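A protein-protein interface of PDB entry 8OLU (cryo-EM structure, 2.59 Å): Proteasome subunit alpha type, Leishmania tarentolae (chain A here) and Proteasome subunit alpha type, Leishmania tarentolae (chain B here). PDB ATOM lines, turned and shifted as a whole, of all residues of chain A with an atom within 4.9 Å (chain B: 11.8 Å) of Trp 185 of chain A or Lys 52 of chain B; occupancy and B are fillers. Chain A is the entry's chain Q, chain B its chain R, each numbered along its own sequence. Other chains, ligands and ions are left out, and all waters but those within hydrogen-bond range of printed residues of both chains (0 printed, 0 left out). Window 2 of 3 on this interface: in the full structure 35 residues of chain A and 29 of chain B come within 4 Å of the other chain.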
ATOM      1  N   VAL A  37      19.975  -1.104   0.043  1.00  0.00           N
ATOM      2  CA  VAL A  37      19.951  -2.534  -0.050  1.00  0.00           C
ATOM      3  C   VAL A  37      20.013  -2.897  -1.499  1.00  0.00           C
ATOM      4  O   VAL A  37      19.073  -2.625  -2.252  1.00  0.00           O
ATOM      5  CB  VAL A  37      18.693  -3.128   0.576  1.00  0.00           C
ATOM      6  CG1 VAL A  37      18.566  -4.574   0.164  1.00  0.00           C
ATOM      7  CG2 VAL A  37      18.746  -3.022   2.080  1.00  0.00           C
ATOM      8  N   CYS A  38      21.077  -3.622  -1.785  1.00  0.00           N
ATOM      9  CA  CYS A  38      21.419  -4.063  -3.118  1.00  0.00           C
ATOM     10  C   CYS A  38      20.983  -5.497  -3.308  1.00  0.00           C
ATOM     11  O   CYS A  38      21.655  -6.379  -2.811  1.00  0.00           O
ATOM     12  CB  CYS A  38      22.922  -3.988  -3.321  1.00  0.00           C
ATOM     13  SG  CYS A  38      23.363  -3.919  -5.063  1.00  0.00           S
ATOM     14  N   SER A 166      26.574  -4.653  -0.274  1.00  0.00           N
ATOM     15  CA  SER A 166      25.349  -5.365  -0.551  1.00  0.00           C
ATOM     16  C   SER A 166      24.233  -4.669   0.188  1.00  0.00           C
ATOM     17  O   SER A 166      23.115  -4.581  -0.259  1.00  0.00           O
ATOM     18  CB  SER A 166      25.510  -6.783  -0.075  1.00  0.00           C
ATOM     19  OG  SER A 166      26.743  -7.374  -0.535  1.00  0.00           O
ATOM     20  N   ALA A 167      24.583  -4.128   1.330  1.00  0.00           N
ATOM     21  CA  ALA A 167      23.675  -3.212   1.961  1.00  0.00           C
ATOM     22  C   ALA A 167      24.472  -2.382   2.922  1.00  0.00           C
ATOM     23  O   ALA A 167      25.548  -2.750   3.293  1.00  0.00           O
ATOM     24  CB  ALA A 167      22.557  -3.950   2.661  1.00  0.00           C
ATOM     25  N   LEU A 181      21.140  -5.137   9.241  1.00  0.00           N
ATOM     26  CA  LEU A 181      21.214  -5.592   7.871  1.00  0.00           C
ATOM     27  C   LEU A 181      22.078  -6.843   7.829  1.00  0.00           C
ATOM     28  O   LEU A 181      21.836  -7.716   7.001  1.00  0.00           O
ATOM     29  CB  LEU A 181      21.854  -4.522   6.985  1.00  0.00           C
ATOM     30  CG  LEU A 181      21.118  -3.193   6.831  1.00  0.00           C
ATOM     31  CD1 LEU A 181      22.051  -2.156   6.199  1.00  0.00           C
ATOM     32  CD2 LEU A 181      19.856  -3.337   5.995  1.00  0.00           C
ATOM     33  N   LYS A 182      23.117  -6.900   8.669  1.00  0.00           N
ATOM     34  CA  LYS A 182      23.993  -8.059   8.745  1.00  0.00           C
ATOM     35  C   LYS A 182      23.109  -9.301   8.840  1.00  0.00           C
ATOM     36  O   LYS A 182      23.232 -10.244   8.063  1.00  0.00           O
ATOM     37  CB  LYS A 182      24.909  -7.940   9.975  1.00  0.00           C
ATOM     38  CG  LYS A 182      26.353  -8.418   9.817  1.00  0.00           C
ATOM     39  CD  LYS A 182      27.374  -7.595  10.631  1.00  0.00           C
ATOM     40  CE  LYS A 182      27.497  -6.145  10.178  1.00  0.00           C
ATOM     41  NZ  LYS A 182      28.294  -5.294  11.099  1.00  0.00           N
ATOM     42  N   LYS A 183      22.160  -9.235   9.771  1.00  0.00           N
ATOM     43  CA  LYS A 183      21.391 -10.383  10.196  1.00  0.00           C
ATOM     44  C   LYS A 183      20.378 -10.792   9.113  1.00  0.00           C
ATOM     45  O   LYS A 183      20.060 -11.970   8.953  1.00  0.00           O
ATOM     46  CB  LYS A 183      20.770  -9.997  11.544  1.00  0.00           C
ATOM     47  CG  LYS A 183      20.415 -11.141  12.485  1.00  0.00           C
ATOM     48  CD  LYS A 183      19.657 -10.678  13.719  1.00  0.00           C
ATOM     49  CE  LYS A 183      18.414  -9.868  13.385  1.00  0.00           C
ATOM     50  NZ  LYS A 183      17.920  -9.095  14.549  1.00  0.00           N
ATOM     51  N   ASP A 184      19.871  -9.832   8.342  1.00  0.00           N
ATOM     52  CA  ASP A 184      18.675 -10.088   7.561  1.00  0.00           C
ATOM     53  C   ASP A 184      18.924 -10.003   6.057  1.00  0.00           C
ATOM     54  O   ASP A 184      18.039 -10.360   5.277  1.00  0.00           O
ATOM     55  CB  ASP A 184      17.541  -9.156   8.008  1.00  0.00           C
ATOM     56  CG  ASP A 184      16.887  -9.513   9.343  1.00  0.00           C
ATOM     57  OD1 ASP A 184      15.796  -8.956   9.614  1.00  0.00           O
ATOM     58  OD2 ASP A 184      17.464 -10.335  10.115  1.00  0.00           O
ATOM     59  N   TRP A 185      20.106  -9.527   5.637  1.00  0.00           N
ATOM     60  CA  TRP A 185      20.434  -9.481   4.215  1.00  0.00           C
ATOM     61  C   TRP A 185      20.839 -10.882   3.784  1.00  0.00           C
ATOM     62  O   TRP A 185      21.460 -11.593   4.574  1.00  0.00           O
ATOM     63  CB  TRP A 185      21.533  -8.442   3.889  1.00  0.00           C
ATOM     64  CG  TRP A 185      21.723  -8.273   2.412  1.00  0.00           C
ATOM     65  CD1 TRP A 185      20.935  -7.562   1.540  1.00  0.00           C
ATOM     66  CD2 TRP A 185      22.684  -8.963   1.598  1.00  0.00           C
ATOM     67  NE1 TRP A 185      21.358  -7.731   0.246  1.00  0.00           N
ATOM     68  CE2 TRP A 185      22.434  -8.580   0.248  1.00  0.00           C
ATOM     69  CE3 TRP A 185      23.730  -9.861   1.888  1.00  0.00           C
ATOM     70  CZ2 TRP A 185      23.202  -9.063  -0.818  1.00  0.00           C
ATOM     71  CZ3 TRP A 185      24.490 -10.337   0.834  1.00  0.00           C
ATOM     72  CH2 TRP A 185      24.222  -9.950  -0.500  1.00  0.00           C
ATOM     73  N   HIS A 186      20.452 -11.271   2.556  1.00  0.00           N
ATOM     74  CA  HIS A 186      21.004 -12.459   1.900  1.00  0.00           C
ATOM     75  C   HIS A 186      21.055 -12.232   0.389  1.00  0.00           C
ATOM     76  O   HIS A 186      20.509 -11.264  -0.111  1.00  0.00           O
ATOM     77  CB  HIS A 186      20.227 -13.747   2.265  1.00  0.00           C
ATOM     78  CG  HIS A 186      18.744 -13.690   2.058  1.00  0.00           C
ATOM     79  ND1 HIS A 186      18.125 -14.026   0.871  1.00  0.00           N
ATOM     80  CD2 HIS A 186      17.763 -13.298   2.927  1.00  0.00           C
ATOM     81  CE1 HIS A 186      16.807 -13.858   1.005  1.00  0.00           C
ATOM     82  NE2 HIS A 186      16.559 -13.401   2.281  1.00  0.00           N
ATOM     83  N   GLU A 187      21.659 -13.170  -0.339  1.00  0.00           N
ATOM     84  CA  GLU A 187      22.148 -12.936  -1.690  1.00  0.00           C
ATOM     85  C   GLU A 187      21.052 -13.069  -2.758  1.00  0.00           C
ATOM     86  O   GLU A 187      21.294 -12.780  -3.925  1.00  0.00           O
ATOM     87  CB  GLU A 187      23.297 -13.921  -1.935  1.00  0.00           C
ATOM     88  CG  GLU A 187      24.328 -13.460  -2.959  1.00  0.00           C
ATOM     89  CD  GLU A 187      25.420 -14.483  -3.251  1.00  0.00           C
ATOM     90  OE1 GLU A 187      26.192 -14.277  -4.214  1.00  0.00           O
ATOM     91  OE2 GLU A 187      25.494 -15.494  -2.516  1.00  0.00           O
ATOM     92  N   MET A 189      17.560 -12.003  -2.698  1.00  0.00           N
ATOM     93  CA  MET A 189      16.385 -11.213  -2.366  1.00  0.00           C
ATOM     94  C   MET A 189      15.672 -10.719  -3.623  1.00  0.00           C
ATOM     95  O   MET A 189      16.301 -10.310  -4.591  1.00  0.00           O
ATOM     96  CB  MET A 189      16.821  -9.980  -1.586  1.00  0.00           C
ATOM     97  CG  MET A 189      17.456 -10.291  -0.275  1.00  0.00           C
ATOM     98  SD  MET A 189      17.679  -8.780   0.716  1.00  0.00           S
ATOM     99  CE  MET A 189      16.031  -8.643   1.408  1.00  0.00           C
ATOM    100  N   LEU A 197      13.267  -5.050   3.826  1.00  0.00           N
ATOM    101  CA  LEU A 197      14.397  -5.062   4.726  1.00  0.00           C
ATOM    102  C   LEU A 197      14.837  -3.636   5.000  1.00  0.00           C
ATOM    103  O   LEU A 197      15.197  -3.290   6.132  1.00  0.00           O
ATOM    104  CB  LEU A 197      15.529  -5.852   4.081  1.00  0.00           C
ATOM    105  CG  LEU A 197      16.860  -5.666   4.781  1.00  0.00           C
ATOM    106  CD1 LEU A 197      16.727  -6.100   6.219  1.00  0.00           C
ATOM    107  CD2 LEU A 197      17.961  -6.429   4.070  1.00  0.00           C
ATOM    108  N   LYS B  48      40.307  -5.868   5.713  1.00  0.00           N
ATOM    109  CA  LYS B  48      39.856  -5.246   6.957  1.00  0.00           C
ATOM    110  C   LYS B  48      39.111  -6.264   7.830  1.00  0.00           C
ATOM    111  O   LYS B  48      39.188  -6.192   9.056  1.00  0.00           O
ATOM    112  CB  LYS B  48      38.999  -4.002   6.676  1.00  0.00           C
ATOM    113  CG  LYS B  48      37.609  -4.298   6.131  1.00  0.00           C
ATOM    114  CD  LYS B  48      36.811  -3.089   5.684  1.00  0.00           C
ATOM    115  CE  LYS B  48      35.420  -3.483   5.220  1.00  0.00           C
ATOM    116  NZ  LYS B  48      34.782  -2.450   4.367  1.00  0.00           N
ATOM    117  N   SER B  49      38.376  -7.177   7.176  1.00  0.00           N
ATOM    118  CA  SER B  49      37.804  -8.378   7.777  1.00  0.00           C
ATOM    119  C   SER B  49      37.004  -9.082   6.679  1.00  0.00           C
ATOM    120  O   SER B  49      37.556  -9.326   5.609  1.00  0.00           O
ATOM    121  CB  SER B  49      36.973  -8.086   9.017  1.00  0.00           C
ATOM    122  OG  SER B  49      36.721  -9.279   9.743  1.00  0.00           O
ATOM    123  N   ALA B  50      35.724  -9.406   6.924  1.00  0.00           N
ATOM    124  CA  ALA B  50      34.779  -9.704   5.850  1.00  0.00           C
ATOM    125  C   ALA B  50      33.356  -9.669   6.403  1.00  0.00           C
ATOM    126  O   ALA B  50      32.726 -10.702   6.621  1.00  0.00           O
ATOM    127  CB  ALA B  50      35.086 -11.030   5.183  1.00  0.00           C
ATOM    128  N   VAL B  51      32.881  -8.446   6.648  1.00  0.00           N
ATOM    129  CA  VAL B  51      31.509  -8.201   7.059  1.00  0.00           C
ATOM    130  C   VAL B  51      30.592  -8.702   5.939  1.00  0.00           C
ATOM    131  O   VAL B  51      30.952  -8.616   4.767  1.00  0.00           O
ATOM    132  CB  VAL B  51      31.331  -6.708   7.436  1.00  0.00           C
ATOM    133  CG1 VAL B  51      31.951  -5.753   6.422  1.00  0.00           C
ATOM    134  CG2 VAL B  51      29.880  -6.339   7.700  1.00  0.00           C
ATOM    135  N   LYS B  52      29.434  -9.277   6.304  1.00  0.00           N
ATOM    136  CA  LYS B  52      28.562  -9.967   5.357  1.00  0.00           C
ATOM    137  C   LYS B  52      27.960  -8.985   4.354  1.00  0.00           C
ATOM    138  O   LYS B  52      27.175  -9.386   3.488  1.00  0.00           O
ATOM    139  CB  LYS B  52      27.407 -10.672   6.079  1.00  0.00           C
ATOM    140  CG  LYS B  52      27.827 -11.748   7.066  1.00  0.00           C
ATOM    141  CD  LYS B  52      26.789 -12.093   8.113  1.00  0.00           C
ATOM    142  CE  LYS B  52      27.386 -12.956   9.208  1.00  0.00           C
ATOM    143  NZ  LYS B  52      26.423 -13.223  10.300  1.00  0.00           N
ATOM    144  N   LEU B  53      28.337  -7.704   4.501  1.00  0.00           N
ATOM    145  CA  LEU B  53      27.696  -6.604   3.802  1.00  0.00           C
ATOM    146  C   LEU B  53      28.521  -6.104   2.631  1.00  0.00           C
ATOM    147  O   LEU B  53      27.945  -5.505   1.740  1.00  0.00           O
ATOM    148  CB  LEU B  53      27.471  -5.456   4.777  1.00  0.00           C
ATOM    149  CG  LEU B  53      26.357  -5.695   5.785  1.00  0.00           C
ATOM    150  CD1 LEU B  53      26.071  -4.398   6.558  1.00  0.00           C
ATOM    151  CD2 LEU B  53      25.114  -6.259   5.091  1.00  0.00           C
ATOM    152  N   GLN B  54      29.843  -6.308   2.642  1.00  0.00           N
ATOM    153  CA  GLN B  54      30.657  -5.791   1.559  1.00  0.00           C
ATOM    154  C   GLN B  54      30.418  -6.691   0.370  1.00  0.00           C
ATOM    155  O   GLN B  54      30.014  -7.837   0.543  1.00  0.00           O
ATOM    156  CB  GLN B  54      32.133  -5.637   1.924  1.00  0.00           C
ATOM    157  CG  GLN B  54      32.942  -6.901   1.714  1.00  0.00           C
ATOM    158  CD  GLN B  54      34.208  -6.837   2.529  1.00  0.00           C
ATOM    159  OE1 GLN B  54      34.611  -5.765   2.984  1.00  0.00           O
ATOM    160  NE2 GLN B  54      34.831  -7.989   2.730  1.00  0.00           N
ATOM    161  N   ASP B  55      30.607  -6.114  -0.823  1.00  0.00           N
ATOM    162  CA  ASP B  55      30.165  -6.766  -2.038  1.00  0.00           C
ATOM    163  C   ASP B  55      31.043  -8.004  -2.250  1.00  0.00           C
ATOM    164  O   ASP B  55      32.287  -7.937  -2.295  1.00  0.00           O
ATOM    165  CB  ASP B  55      30.098  -5.810  -3.227  1.00  0.00           C
ATOM    166  CG  ASP B  55      28.963  -6.124  -4.192  1.00  0.00           C
ATOM    167  OD1 ASP B  55      29.254  -6.435  -5.363  1.00  0.00           O
ATOM    168  OD2 ASP B  55      27.780  -6.040  -3.769  1.00  0.00           O
ATOM    169  N   SER B  56      30.315  -9.137  -2.332  1.00  0.00           N
ATOM    170  CA  SER B  56      30.849 -10.477  -2.509  1.00  0.00           C
ATOM    171  C   SER B  56      31.487 -10.630  -3.895  1.00  0.00           C
ATOM    172  O   SER B  56      32.208 -11.600  -4.140  1.00  0.00           O
ATOM    173  CB  SER B  56      29.765 -11.516  -2.228  1.00  0.00           C
ATOM    174  OG  SER B  56      28.470 -11.051  -2.600  1.00  0.00           O
ATOM    175  N   ARG B  57      31.221  -9.663  -4.794  1.00  0.00           N
ATOM    176  CA  ARG B  57      32.050  -9.424  -5.969  1.00  0.00           C
ATOM    177  C   ARG B  57      33.458  -8.999  -5.533  1.00  0.00           C
ATOM    178  O   ARG B  57      33.644  -8.187  -4.620  1.00  0.00           O
ATOM    179  CB  ARG B  57      31.413  -8.389  -6.905  1.00  0.00           C
ATOM    180  CG  ARG B  57      32.432  -7.685  -7.789  1.00  0.00           C
ATOM    181  CD  ARG B  57      31.943  -6.390  -8.409  1.00  0.00           C
ATOM    182  NE  ARG B  57      31.706  -5.291  -7.472  1.00  0.00           N
ATOM    183  CZ  ARG B  57      32.019  -4.009  -7.673  1.00  0.00           C
ATOM    184  NH1 ARG B  57      31.167  -3.079  -7.271  1.00  0.00           N
ATOM    185  NH2 ARG B  57      33.140  -3.658  -8.292  1.00  0.00           N
ATOM    186  N   THR B  58      34.451  -9.576  -6.217  1.00  0.00           N
ATOM    187  CA  THR B  58      35.846  -9.445  -5.829  1.00  0.00           C
ATOM    188  C   THR B  58      36.288  -7.996  -6.059  1.00  0.00           C
ATOM    189  O   THR B  58      36.226  -7.480  -7.175  1.00  0.00           O
ATOM    190  CB  THR B  58      36.715 -10.532  -6.495  1.00  0.00           C
ATOM    191  OG1 THR B  58      38.081 -10.141  -6.344  1.00  0.00           O
ATOM    192  CG2 THR B  58      36.428 -10.780  -7.965  1.00  0.00           C
ATOM    193  N   SER B 201      41.772 -16.434   7.165  1.00  0.00           N
ATOM    194  CA  SER B 201      40.534 -16.901   6.574  1.00  0.00           C
ATOM    195  C   SER B 201      40.157 -15.976   5.420  1.00  0.00           C
ATOM    196  O   SER B 201      40.503 -16.253   4.268  1.00  0.00           O
ATOM    197  CB  SER B 201      39.462 -17.001   7.649  1.00  0.00           C
ATOM    198  OG  SER B 201      38.193 -17.300   7.093  1.00  0.00           O
ATOM    199  N   ARG B 202      39.494 -14.860   5.758  1.00  0.00           N
ATOM    200  CA  ARG B 202      38.947 -13.940   4.774  1.00  0.00           C
ATOM    201  C   ARG B 202      39.693 -12.608   4.819  1.00  0.00           C
ATOM    202  O   ARG B 202      39.274 -11.652   4.167  1.00  0.00           O
ATOM    203  CB  ARG B 202      37.450 -13.724   5.026  1.00  0.00           C
ATOM    204  CG  ARG B 202      36.547 -14.760   4.369  1.00  0.00           C
ATOM    205  CD  ARG B 202      35.111 -14.678   4.856  1.00  0.00           C
ATOM    206  NE  ARG B 202      34.258 -15.677   4.223  1.00  0.00           N
ATOM    207  CZ  ARG B 202      33.055 -16.042   4.659  1.00  0.00           C
ATOM    208  NH1 ARG B 202      32.643 -15.678   5.860  1.00  0.00           N
ATOM    209  NH2 ARG B 202      32.276 -16.790   3.896  1.00  0.00           N
ATOM    210  N   GLU B 219      40.080 -17.944  -3.052  1.00  0.00           N
ATOM    211  CA  GLU B 219      39.998 -18.072  -1.602  1.00  0.00           C
ATOM    212  C   GLU B 219      40.245 -19.530  -1.183  1.00  0.00           C
ATOM    213  O   GLU B 219      40.609 -19.785  -0.034  1.00  0.00           O
ATOM    214  CB  GLU B 219      38.669 -17.503  -1.100  1.00  0.00           C
ATOM    215  CG  GLU B 219      38.667 -17.203   0.395  1.00  0.00           C
ATOM    216  CD  GLU B 219      37.368 -16.623   0.941  1.00  0.00           C
ATOM    217  OE1 GLU B 219      37.054 -15.459   0.612  1.00  0.00           O
ATOM    218  OE2 GLU B 219      36.664 -17.338   1.690  1.00  0.00           O
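Among the printed residues, merely in contact across the chains: Lys 182 of chain A with Val 51 of chain B (3.4 Å), Ala 167 of chain A with Leu 53 of chain B (3.6 Å), Ser 166 of chain A with Asp 55 of chain B (3.6 Å) and Trp 185 of chain A with Lys 52 of chain B (3.8 Å).
No residue of chain B comes within 4 Å of Val 37 of chain A.
Printed residues of chain B within 4 Å of Ser 166 of chain A: Leu 53, Gln 54 and Asp 55.
No residue of chain B comes within 4 Å of Leu 181 of chain A.
Of the printed residues of chain B, Lys 182 of chain A touches Val 51.
Lys 183 of chain A touches none of the printed residues of chain B.
Trp 185 of chain A touches just one residue of chain B: Lys 52.
No residue of chain B comes within 4 Å of His 186 of chain A.
No residue of chain B comes within 4 Å of Met 189 of chain A.
Of the printed residues of chain A, Val 51 of chain B touches Lys 182 (3.4 Å).
Printed residues of chain A within 4 Å of Lys 52 of chain B: Trp 185 (3.8 Å).
Of the printed residues of chain A, Leu 53 of chain B touches Ser 166 (2.6 Å) and Ala 167 (3.6 Å).
Printed residues of chain A within 4 Å of Gln 54 of chain B: Ser 166.
Printed residues of chain A within 4 Å of Asp 55 of chain B: Ser 166 (3.6 Å).
Thr 58 of chain B touches none of the printed residues of chain A.
The nearest residue of chain B that does not touch Trp 185 of chain A is Leu 53 of chain B (4.4 Å).
The nearest printed residue of chain B that does not touch Lys 182 of chain A is Lys 52 of chain B (4.01 Å).
Printed residues of chain A that touch a printed residue of chain B: Ser 166, Ala 167, Lys 182 and Trp 185.
Hydrophobic or aromatic side chains of chain A within 4 Å of the printed part of chain B: Trp 185.
Hydrophobic or aromatic side chains of chain B that line the printed part of chain A: Val 51 and Leu 53.
Among the printed residues, 6 pairs touch across the chains.
OG of Ser 166 of chain A lies within hydrogen-bond range of O of Gln 54 of chain B, 3.5 Å away.
The backbone carbonyl oxygen (O) of Leu 53 of chain B is in hydrogen-bond range of the backbone NH (N) of Ser 166 of chain A, at 2.6 Å.
O of Ser 166 of chain A sits at hydrogen-bond distance from N of Cys 38 of chain A, at 2.7 Å.
NE1 of Trp 185 of chain A is in hydrogen-bond range of O of Cys 38 of chain A, 3.4 Å away.
The side-chain carboxylate (OD1) of Asp 55 of chain B lies within salt-bridge range of the guanidinium group (NE) of Arg 57 of chain B.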
